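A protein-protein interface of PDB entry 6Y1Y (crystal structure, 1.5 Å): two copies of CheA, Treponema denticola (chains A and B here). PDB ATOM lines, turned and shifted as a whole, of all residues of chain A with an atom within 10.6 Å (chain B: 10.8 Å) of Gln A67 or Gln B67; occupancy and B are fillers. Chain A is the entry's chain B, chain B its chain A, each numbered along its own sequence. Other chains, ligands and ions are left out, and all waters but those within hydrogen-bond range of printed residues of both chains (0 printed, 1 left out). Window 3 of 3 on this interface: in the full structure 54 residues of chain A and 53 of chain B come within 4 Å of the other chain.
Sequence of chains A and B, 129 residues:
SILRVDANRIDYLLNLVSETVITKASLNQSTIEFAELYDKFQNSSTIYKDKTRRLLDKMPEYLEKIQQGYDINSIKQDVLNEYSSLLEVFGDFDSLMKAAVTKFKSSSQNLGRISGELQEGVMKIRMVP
Hydrophobic or aromatic side chains of chain A within 4 Å of the printed part of chain B: Met A59, Leu A63 and Ile A66. Of the 15 printed residues of chain B, 7 touch a printed residue of chain A. Among the printed residues, 12 pairs touch across the chains. Among the printed residues, no Asp or Glu carboxylate lies within 4 Å of a Lys or Arg side-chain nitrogen of the other chain.
Met A59 touches Tyr B62, but with the chains exchanged Tyr A62 does not touch Met B59 (4.05 Å). Leu A63 touches Met B59, but with the chains exchanged Met A59 does not touch Leu B63 (7.8 Å). Ile A66 touches Leu B63, but with the chains exchanged Leu A63 does not touch Ile B66 (4.5 Å). Gln A67 touches Leu B63, but with the chains exchanged Leu A63 does not touch Gln B67 (7.2 Å). Positions printed for both chains: 59, 60, 61, 62, 63, 64, 65, 66, 67, 68, 69, 70, 71, 72 and 75. Of the 12 pairs that touch across the chains among the printed residues, 3 have their exchanged pair printed and touching as well.
Among the printed residues, merely in contact across the chains: Gln A67 with Ile B66, Gln A67 with Gln B67, Pro A60 with Ile B72, Leu A63 with Tyr B62, Leu A63 with Leu B63, Leu A63 with Ile B75, Ile A66 with Leu B63, Glu A64 with Ile B72, Met A59 with Met B59, Met A59 with Tyr B62, Leu A63 with Met B59 and Gln A67 with Leu B63.
Of the printed residues of chain B, Met A59 touches Met B59 and Tyr B62. Printed residues of chain B within 4 Å of Glu A64: Ile B72. Lys A65 touches none of the printed residues of chain B. Of chain B, only Leu B63 (3.8 Å) comes within 4 Å of Ile A66. Of the printed residues of chain B, Gln A67 touches Leu B63 (3.98 Å), Ile B66 (3.3 Å) and Gln B67 (3.3 Å). No residue of chain B comes within 4 Å of Gln A68. No residue of chain B comes within 4 Å of Gly A69. Glu B61 touches none of the printed residues of chain A. Printed residues of chain A within 4 Å of Tyr B62: Met A59 (3.9 Å) and Leu A63 (3.6 Å). Ile B66 touches one residue of chain A. Of chain A, only Gln A67 comes within 4 Å of Gln B67. Of the printed residues of chain A, Ile B72 touches Pro A60 (3.5 Å) and Glu A64 (3.8 Å). Printed residues of chain A within 4 Å of Ile B75: Leu A63. The nearest printed residue of chain B that does not touch Gln A67 is Gln B68 (5.9 Å). The nearest residue of chain A that does not touch Gln B67 is Ile A66 (5.1 Å). The nearest printed residue of chain B that does not touch Pro A60 is Ile B75 (4.9 Å).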
ATOM      1  N   MET A  59      -0.544  10.682  17.969  1.00  0.00           N
ATOM      2  CA  MET A  59       0.396   9.578  18.146  1.00  0.00           C
ATOM      3  C   MET A  59       1.615   9.982  18.956  1.00  0.00           C
ATOM      4  O   MET A  59       1.900   9.302  19.962  1.00  0.00           O
ATOM      5  CB  MET A  59       0.803   8.972  16.801  1.00  0.00           C
ATOM      6  CG  MET A  59       1.615   7.696  17.037  1.00  0.00           C
ATOM      7  SD  MET A  59       1.991   6.660  15.615  1.00  0.00           S
ATOM      8  CE  MET A  59       0.419   5.805  15.435  1.00  0.00           C
ATOM      9  N   PRO A  60       2.324  11.071  18.653  1.00  0.00           N
ATOM     10  CA  PRO A  60       3.468  11.435  19.503  1.00  0.00           C
ATOM     11  C   PRO A  60       3.045  11.864  20.891  1.00  0.00           C
ATOM     12  O   PRO A  60       3.725  11.539  21.875  1.00  0.00           O
ATOM     13  CB  PRO A  60       4.148  12.581  18.732  1.00  0.00           C
ATOM     14  CG  PRO A  60       3.593  12.508  17.336  1.00  0.00           C
ATOM     15  CD  PRO A  60       2.199  11.981  17.497  1.00  0.00           C
ATOM     16  N   GLU A  61       1.900  12.535  21.006  1.00  0.00           N
ATOM     17  CA  GLU A  61       1.412  12.935  22.319  1.00  0.00           C
ATOM     18  C   GLU A  61       1.134  11.718  23.179  1.00  0.00           C
ATOM     19  O   GLU A  61       1.503  11.682  24.360  1.00  0.00           O
ATOM     20  CB  GLU A  61       0.138  13.771  22.165  1.00  0.00           C
ATOM     21  CG  GLU A  61       0.332  15.124  21.515  1.00  0.00           C
ATOM     22  CD  GLU A  61       0.565  16.214  22.541  1.00  0.00           C
ATOM     23  OE1 GLU A  61       0.782  17.376  22.134  1.00  0.00           O
ATOM     24  OE2 GLU A  61       0.527  15.903  23.755  1.00  0.00           O
ATOM     25  N   TYR A  62       0.508  10.701  22.593  1.00  0.00           N
ATOM     26  CA  TYR A  62       0.167   9.494  23.337  1.00  0.00           C
ATOM     27  C   TYR A  62       1.402   8.704  23.741  1.00  0.00           C
ATOM     28  O   TYR A  62       1.403   8.067  24.796  1.00  0.00           O
ATOM     29  CB  TYR A  62      -0.800   8.640  22.526  1.00  0.00           C
ATOM     30  CG  TYR A  62      -2.224   9.139  22.593  1.00  0.00           C
ATOM     31  CD1 TYR A  62      -2.538  10.351  23.202  1.00  0.00           C
ATOM     32  CD2 TYR A  62      -3.248   8.392  22.046  1.00  0.00           C
ATOM     33  CE1 TYR A  62      -3.848  10.800  23.267  1.00  0.00           C
ATOM     34  CE2 TYR A  62      -4.561   8.826  22.105  1.00  0.00           C
ATOM     35  CZ  TYR A  62      -4.849  10.029  22.722  1.00  0.00           C
ATOM     36  OH  TYR A  62      -6.154  10.468  22.794  1.00  0.00           O
ATOM     37  N   LEU A  63       2.438   8.685  22.897  1.00  0.00           N
ATOM     38  CA  LEU A  63       3.681   8.030  23.295  1.00  0.00           C
ATOM     39  C   LEU A  63       4.260   8.701  24.526  1.00  0.00           C
ATOM     40  O   LEU A  63       4.695   8.027  25.470  1.00  0.00           O
ATOM     41  CB  LEU A  63       4.690   8.081  22.147  1.00  0.00           C
ATOM     42  CG  LEU A  63       4.319   7.268  20.915  1.00  0.00           C
ATOM     43  CD1 LEU A  63       5.177   7.660  19.703  1.00  0.00           C
ATOM     44  CD2 LEU A  63       4.434   5.787  21.232  1.00  0.00           C
ATOM     45  N   GLU A  64       4.272  10.036  24.532  1.00  0.00           N
ATOM     46  CA  GLU A  64       4.715  10.771  25.712  1.00  0.00           C
ATOM     47  C   GLU A  64       3.878  10.407  26.934  1.00  0.00           C
ATOM     48  O   GLU A  64       4.413  10.215  28.030  1.00  0.00           O
ATOM     49  CB  GLU A  64       4.644  12.272  25.438  1.00  0.00           C
ATOM     50  CG  GLU A  64       5.373  13.139  26.440  1.00  0.00           C
ATOM     51  CD  GLU A  64       5.811  14.456  25.828  1.00  0.00           C
ATOM     52  OE1 GLU A  64       4.926  15.263  25.462  1.00  0.00           O
ATOM     53  OE2 GLU A  64       7.034  14.683  25.714  1.00  0.00           O
ATOM     54  N   LYS A  65       2.561  10.292  26.764  1.00  0.00           N
ATOM     55  CA  LYS A  65       1.700   9.983  27.901  1.00  0.00           C
ATOM     56  C   LYS A  65       1.964   8.580  28.441  1.00  0.00           C
ATOM     57  O   LYS A  65       1.874   8.352  29.652  1.00  0.00           O
ATOM     58  CB  LYS A  65       0.238  10.193  27.520  1.00  0.00           C
ATOM     59  CG  LYS A  65      -0.061  11.672  27.295  1.00  0.00           C
ATOM     60  CD  LYS A  65      -1.459  11.907  26.785  1.00  0.00           C
ATOM     61  CE  LYS A  65      -1.965  13.282  27.192  1.00  0.00           C
ATOM     62  NZ  LYS A  65      -1.085  13.909  28.217  1.00  0.00           N
ATOM     63  N   ILE A  66       2.243   7.611  27.567  1.00  0.00           N
ATOM     64  CA  ILE A  66       2.618   6.290  28.057  1.00  0.00           C
ATOM     65  C   ILE A  66       3.861   6.396  28.937  1.00  0.00           C
ATOM     66  O   ILE A  66       3.933   5.792  30.018  1.00  0.00           O
ATOM     67  CB  ILE A  66       2.837   5.323  26.877  1.00  0.00           C
ATOM     68  CG1 ILE A  66       1.502   4.968  26.215  1.00  0.00           C
ATOM     69  CG2 ILE A  66       3.559   4.059  27.339  1.00  0.00           C
ATOM     70  CD1 ILE A  66       1.658   4.289  24.867  1.00  0.00           C
ATOM     71  N   GLN A  67       4.838   7.198  28.506  1.00  0.00           N
ATOM     72  CA  GLN A  67       6.062   7.388  29.281  1.00  0.00           C
ATOM     73  C   GLN A  67       5.805   8.104  30.593  1.00  0.00           C
ATOM     74  O   GLN A  67       6.541   7.898  31.568  1.00  0.00           O
ATOM     75  CB  GLN A  67       7.080   8.177  28.469  1.00  0.00           C
ATOM     76  CG  GLN A  67       7.826   7.333  27.505  1.00  0.00           C
ATOM     77  CD  GLN A  67       8.283   6.023  28.105  1.00  0.00           C
ATOM     78  OE1 GLN A  67       7.626   4.994  27.940  1.00  0.00           O
ATOM     79  NE2 GLN A  67       9.410   6.051  28.806  1.00  0.00           N
ATOM     80  N   GLN A  68       4.788   8.954  30.638  1.00  0.00           N
ATOM     81  CA  GLN A  68       4.442   9.642  31.869  1.00  0.00           C
ATOM     82  C   GLN A  68       3.596   8.783  32.801  1.00  0.00           C
ATOM     83  O   GLN A  68       3.228   9.251  33.883  1.00  0.00           O
ATOM     84  CB  GLN A  68       3.725  10.956  31.542  1.00  0.00           C
ATOM     85  CG  GLN A  68       4.605  11.931  30.759  1.00  0.00           C
ATOM     86  CD  GLN A  68       3.829  13.077  30.139  1.00  0.00           C
ATOM     87  OE1 GLN A  68       2.601  13.110  30.186  1.00  0.00           O
ATOM     88  NE2 GLN A  68       4.549  14.033  29.559  1.00  0.00           N
ATOM     89  N   GLY A  69       3.304   7.539  32.428  1.00  0.00           N
ATOM     90  CA  GLY A  69       2.589   6.632  33.299  1.00  0.00           C
ATOM     91  C   GLY A  69       1.091   6.535  33.112  1.00  0.00           C
ATOM     92  O   GLY A  69       0.420   5.973  33.983  1.00  0.00           O
ATOM     93  N   TYR A  70       0.541   7.078  32.030  1.00  0.00           N
ATOM     94  CA  TYR A  70      -0.892   6.977  31.773  1.00  0.00           C
ATOM     95  C   TYR A  70      -1.320   5.519  31.597  1.00  0.00           C
ATOM     96  O   TYR A  70      -0.512   4.634  31.297  1.00  0.00           O
ATOM     97  CB  TYR A  70      -1.271   7.764  30.515  1.00  0.00           C
ATOM     98  CG  TYR A  70      -1.552   9.239  30.715  1.00  0.00           C
ATOM     99  CD1 TYR A  70      -0.572  10.105  31.185  1.00  0.00           C
ATOM    100  CD2 TYR A  70      -2.796   9.773  30.393  1.00  0.00           C
ATOM    101  CE1 TYR A  70      -0.828  11.461  31.342  1.00  0.00           C
ATOM    102  CE2 TYR A  70      -3.058  11.117  30.544  1.00  0.00           C
ATOM    103  CZ  TYR A  70      -2.075  11.958  31.021  1.00  0.00           C
ATOM    104  OH  TYR A  70      -2.354  13.301  31.170  1.00  0.00           O
ATOM    105  N   ASP A  71      -2.606   5.261  31.836  1.00  0.00           N
ATOM    106  CA  ASP A  71      -3.159   3.935  31.574  1.00  0.00           C
ATOM    107  C   ASP A  71      -2.940   3.592  30.099  1.00  0.00           C
ATOM    108  O   ASP A  71      -3.484   4.262  29.208  1.00  0.00           O
ATOM    109  CB  ASP A  71      -4.650   3.933  31.932  1.00  0.00           C
ATOM    110  CG  ASP A  71      -5.312   2.563  31.789  1.00  0.00           C
ATOM    111  OD1 ASP A  71      -4.994   1.808  30.846  1.00  0.00           O
ATOM    112  OD2 ASP A  71      -6.186   2.245  32.624  1.00  0.00           O
ATOM    113  N   ILE A  72      -2.140   2.549  29.843  1.00  0.00           N
ATOM    114  CA  ILE A  72      -1.760   2.223  28.470  1.00  0.00           C
ATOM    115  C   ILE A  72      -2.929   1.660  27.659  1.00  0.00           C
ATOM    116  O   ILE A  72      -3.008   1.879  26.451  1.00  0.00           O
ATOM    117  CB  ILE A  72      -0.549   1.279  28.434  1.00  0.00           C
ATOM    118  CG1 ILE A  72       0.176   1.424  27.095  1.00  0.00           C
ATOM    119  CG2 ILE A  72      -0.958  -0.160  28.636  1.00  0.00           C
ATOM    120  CD1 ILE A  72       1.636   1.087  27.133  1.00  0.00           C
ATOM    121  N   ILE A  75      -4.827   4.436  26.039  1.00  0.00           N
ATOM    122  CA  ILE A  75      -4.112   4.954  24.879  1.00  0.00           C
ATOM    123  C   ILE A  75      -4.314   4.044  23.675  1.00  0.00           C
ATOM    124  O   ILE A  75      -4.714   4.492  22.596  1.00  0.00           O
ATOM    125  CB  ILE A  75      -2.620   5.113  25.225  1.00  0.00           C
ATOM    126  CG1 ILE A  75      -2.439   6.140  26.348  1.00  0.00           C
ATOM    127  CG2 ILE A  75      -1.817   5.422  23.972  1.00  0.00           C
ATOM    128  CD1 ILE A  75      -2.409   7.561  25.874  1.00  0.00           C
ATOM    129  N   MET B  59       3.581   2.103  15.680  1.00  0.00           N
ATOM    130  CA  MET B  59       3.569   2.799  16.966  1.00  0.00           C
ATOM    131  C   MET B  59       4.389   2.086  18.043  1.00  0.00           C
ATOM    132  O   MET B  59       5.079   2.786  18.805  1.00  0.00           O
ATOM    133  CB  MET B  59       2.124   3.022  17.437  1.00  0.00           C
ATOM    134  CG  MET B  59       2.020   3.938  18.655  1.00  0.00           C
ATOM    135  SD  MET B  59       0.312   4.391  19.042  1.00  0.00           S
ATOM    136  CE  MET B  59       0.548   5.395  20.516  1.00  0.00           C
ATOM    137  N   PRO B  60       4.362   0.754  18.179  1.00  0.00           N
ATOM    138  CA  PRO B  60       5.209   0.127  19.209  1.00  0.00           C
ATOM    139  C   PRO B  60       6.700   0.326  18.976  1.00  0.00           C
ATOM    140  O   PRO B  60       7.468   0.324  19.956  1.00  0.00           O
ATOM    141  CB  PRO B  60       4.819  -1.356  19.142  1.00  0.00           C
ATOM    142  CG  PRO B  60       3.496  -1.384  18.483  1.00  0.00           C
ATOM    143  CD  PRO B  60       3.485  -0.231  17.526  1.00  0.00           C
ATOM    144  N   GLU B  61       7.158   0.424  17.723  1.00  0.00           N
ATOM    145  CA  GLU B  61       8.573   0.734  17.487  1.00  0.00           C
ATOM    146  C   GLU B  61       8.894   2.140  17.958  1.00  0.00           C
ATOM    147  O   GLU B  61       9.936   2.372  18.589  1.00  0.00           O
ATOM    148  CB  GLU B  61       8.948   0.583  16.015  1.00  0.00           C
ATOM    149  CG  GLU B  61      10.445   0.816  15.813  1.00  0.00           C
ATOM    150  CD  GLU B  61      10.880   0.845  14.365  1.00  0.00           C
ATOM    151  OE1 GLU B  61      10.048   0.555  13.480  1.00  0.00           O
ATOM    152  OE2 GLU B  61      12.064   1.163  14.124  1.00  0.00           O
ATOM    153  N   TYR B  62       8.007   3.094  17.670  1.00  0.00           N
ATOM    154  CA  TYR B  62       8.216   4.440  18.178  1.00  0.00           C
ATOM    155  C   TYR B  62       8.246   4.431  19.708  1.00  0.00           C
ATOM    156  O   TYR B  62       9.081   5.108  20.326  1.00  0.00           O
ATOM    157  CB  TYR B  62       7.100   5.369  17.690  1.00  0.00           C
ATOM    158  CG  TYR B  62       7.001   5.665  16.204  1.00  0.00           C
ATOM    159  CD1 TYR B  62       8.133   5.804  15.400  1.00  0.00           C
ATOM    160  CD2 TYR B  62       5.755   5.847  15.612  1.00  0.00           C
ATOM    161  CE1 TYR B  62       8.013   6.117  14.035  1.00  0.00           C
ATOM    162  CE2 TYR B  62       5.629   6.143  14.262  1.00  0.00           C
ATOM    163  CZ  TYR B  62       6.755   6.295  13.484  1.00  0.00           C
ATOM    164  OH  TYR B  62       6.611   6.603  12.134  1.00  0.00           O
ATOM    165  N   LEU B  63       7.382   3.625  20.334  1.00  0.00           N
ATOM    166  CA  LEU B  63       7.383   3.518  21.788  1.00  0.00           C
ATOM    167  C   LEU B  63       8.685   2.928  22.301  1.00  0.00           C
ATOM    168  O   LEU B  63       9.230   3.404  23.304  1.00  0.00           O
ATOM    169  CB  LEU B  63       6.201   2.685  22.270  1.00  0.00           C
ATOM    170  CG  LEU B  63       6.133   2.550  23.798  1.00  0.00           C
ATOM    171  CD1 LEU B  63       6.012   3.905  24.466  1.00  0.00           C
ATOM    172  CD2 LEU B  63       4.938   1.667  24.161  1.00  0.00           C
ATOM    173  N   GLU B  64       9.198   1.886  21.639  1.00  0.00           N
ATOM    174  CA  GLU B  64      10.476   1.322  22.064  1.00  0.00           C
ATOM    175  C   GLU B  64      11.570   2.380  22.064  1.00  0.00           C
ATOM    176  O   GLU B  64      12.362   2.463  23.014  1.00  0.00           O
ATOM    177  CB  GLU B  64      10.882   0.160  21.166  1.00  0.00           C
ATOM    178  CG  GLU B  64      12.194  -0.462  21.614  1.00  0.00           C
ATOM    179  CD  GLU B  64      12.225  -1.959  21.441  1.00  0.00           C
ATOM    180  OE1 GLU B  64      11.579  -2.672  22.252  1.00  0.00           O
ATOM    181  OE2 GLU B  64      12.909  -2.415  20.505  1.00  0.00           O
ATOM    182  N   LYS B  65      11.618   3.213  21.026  1.00  0.00           N
ATOM    183  CA  LYS B  65      12.654   4.239  20.979  1.00  0.00           C
ATOM    184  C   LYS B  65      12.469   5.253  22.095  1.00  0.00           C
ATOM    185  O   LYS B  65      13.436   5.611  22.776  1.00  0.00           O
ATOM    186  CB  LYS B  65      12.638   4.962  19.633  1.00  0.00           C
ATOM    187  CG  LYS B  65      12.955   4.095  18.433  1.00  0.00           C
ATOM    188  CD  LYS B  65      13.220   4.959  17.222  1.00  0.00           C
ATOM    189  CE  LYS B  65      13.791   4.135  16.111  1.00  0.00           C
ATOM    190  NZ  LYS B  65      14.041   4.989  14.896  1.00  0.00           N
ATOM    191  N   ILE B  66      11.229   5.693  22.323  1.00  0.00           N
ATOM    192  CA  ILE B  66      10.948   6.642  23.402  1.00  0.00           C
ATOM    193  C   ILE B  66      11.336   6.047  24.752  1.00  0.00           C
ATOM    194  O   ILE B  66      11.870   6.743  25.629  1.00  0.00           O
ATOM    195  CB  ILE B  66       9.468   7.069  23.356  1.00  0.00           C
ATOM    196  CG1 ILE B  66       9.194   7.869  22.087  1.00  0.00           C
ATOM    197  CG2 ILE B  66       9.135   7.943  24.525  1.00  0.00           C
ATOM    198  CD1 ILE B  66       9.931   9.180  22.047  1.00  0.00           C
ATOM    199  N   GLN B  67      11.073   4.753  24.942  1.00  0.00           N
ATOM    200  CA  GLN B  67      11.432   4.099  26.199  1.00  0.00           C
ATOM    201  C   GLN B  67      12.933   4.090  26.413  1.00  0.00           C
ATOM    202  O   GLN B  67      13.400   4.070  27.563  1.00  0.00           O
ATOM    203  CB  GLN B  67      10.895   2.665  26.219  1.00  0.00           C
ATOM    204  CG  GLN B  67       9.400   2.605  26.405  1.00  0.00           C
ATOM    205  CD  GLN B  67       8.845   1.203  26.284  1.00  0.00           C
ATOM    206  OE1 GLN B  67       9.503   0.294  25.789  1.00  0.00           O
ATOM    207  NE2 GLN B  67       7.621   1.024  26.748  1.00  0.00           N
ATOM    208  N   GLN B  68      13.697   4.076  25.330  1.00  0.00           N
ATOM    209  CA  GLN B  68      15.147   4.158  25.385  1.00  0.00           C
ATOM    210  C   GLN B  68      15.659   5.590  25.481  1.00  0.00           C
ATOM    211  O   GLN B  68      16.878   5.796  25.495  1.00  0.00           O
ATOM    212  CB  GLN B  68      15.722   3.454  24.160  1.00  0.00           C
ATOM    213  CG  GLN B  68      15.372   1.976  24.148  1.00  0.00           C
ATOM    214  CD  GLN B  68      15.847   1.267  22.904  1.00  0.00           C
ATOM    215  OE1 GLN B  68      16.332   1.896  21.960  1.00  0.00           O
ATOM    216  NE2 GLN B  68      15.726  -0.053  22.897  1.00  0.00           N
ATOM    217  N   GLY B  69      14.770   6.572  25.555  1.00  0.00           N
ATOM    218  CA  GLY B  69      15.140   7.960  25.716  1.00  0.00           C
ATOM    219  C   GLY B  69      15.224   8.756  24.439  1.00  0.00           C
ATOM    220  O   GLY B  69      15.670   9.909  24.479  1.00  0.00           O
ATOM    221  N   TYR B  70      14.772   8.200  23.317  1.00  0.00           N
ATOM    222  CA  TYR B  70      14.827   8.924  22.055  1.00  0.00           C
ATOM    223  C   TYR B  70      13.987  10.194  22.135  1.00  0.00           C
ATOM    224  O   TYR B  70      12.906  10.205  22.733  1.00  0.00           O
ATOM    225  CB  TYR B  70      14.310   8.022  20.939  1.00  0.00           C
ATOM    226  CG  TYR B  70      14.705   8.395  19.538  1.00  0.00           C
ATOM    227  CD1 TYR B  70      16.033   8.683  19.208  1.00  0.00           C
ATOM    228  CD2 TYR B  70      13.752   8.432  18.530  1.00  0.00           C
ATOM    229  CE1 TYR B  70      16.388   9.013  17.908  1.00  0.00           C
ATOM    230  CE2 TYR B  70      14.099   8.748  17.225  1.00  0.00           C
ATOM    231  CZ  TYR B  70      15.417   9.037  16.922  1.00  0.00           C
ATOM    232  OH  TYR B  70      15.754   9.359  15.622  1.00  0.00           O
ATOM    233  N   ASP B  71      14.461  11.248  21.480  1.00  0.00           N
ATOM    234  CA  ASP B  71      13.776  12.538  21.469  1.00  0.00           C
ATOM    235  C   ASP B  71      12.387  12.439  20.847  1.00  0.00           C
ATOM    236  O   ASP B  71      12.249  12.057  19.683  1.00  0.00           O
ATOM    237  CB  ASP B  71      14.636  13.549  20.702  1.00  0.00           C
ATOM    238  CG  ASP B  71      14.154  14.989  20.840  1.00  0.00           C
ATOM    239  OD1 ASP B  71      13.018  15.231  21.300  1.00  0.00           O
ATOM    240  OD2 ASP B  71      14.929  15.892  20.455  1.00  0.00           O
ATOM    241  N   ILE B  72      11.358  12.837  21.602  1.00  0.00           N
ATOM    242  CA  ILE B  72       9.993  12.771  21.082  1.00  0.00           C
ATOM    243  C   ILE B  72       9.840  13.640  19.838  1.00  0.00           C
ATOM    244  O   ILE B  72       9.055  13.318  18.936  1.00  0.00           O
ATOM    245  CB  ILE B  72       8.989  13.178  22.186  1.00  0.00           C
ATOM    246  CG1 ILE B  72       7.554  12.970  21.699  1.00  0.00           C
ATOM    247  CG2 ILE B  72       9.194  14.637  22.604  1.00  0.00           C
ATOM    248  CD1 ILE B  72       7.236  11.525  21.385  1.00  0.00           C
ATOM    249  N   ILE B  75      10.721  11.592  16.938  1.00  0.00           N
ATOM    250  CA  ILE B  75       9.600  10.719  16.591  1.00  0.00           C
ATOM    251  C   ILE B  75       8.559  11.489  15.798  1.00  0.00           C
ATOM    252  O   ILE B  75       8.053  11.007  14.777  1.00  0.00           O
ATOM    253  CB  ILE B  75       8.991  10.093  17.851  1.00  0.00           C
ATOM    254  CG1 ILE B  75       9.977   9.083  18.455  1.00  0.00           C
ATOM    255  CG2 ILE B  75       7.657   9.432  17.512  1.00  0.00           C
ATOM    256  CD1 ILE B  75      10.178   7.827  17.600  1.00  0.00           C
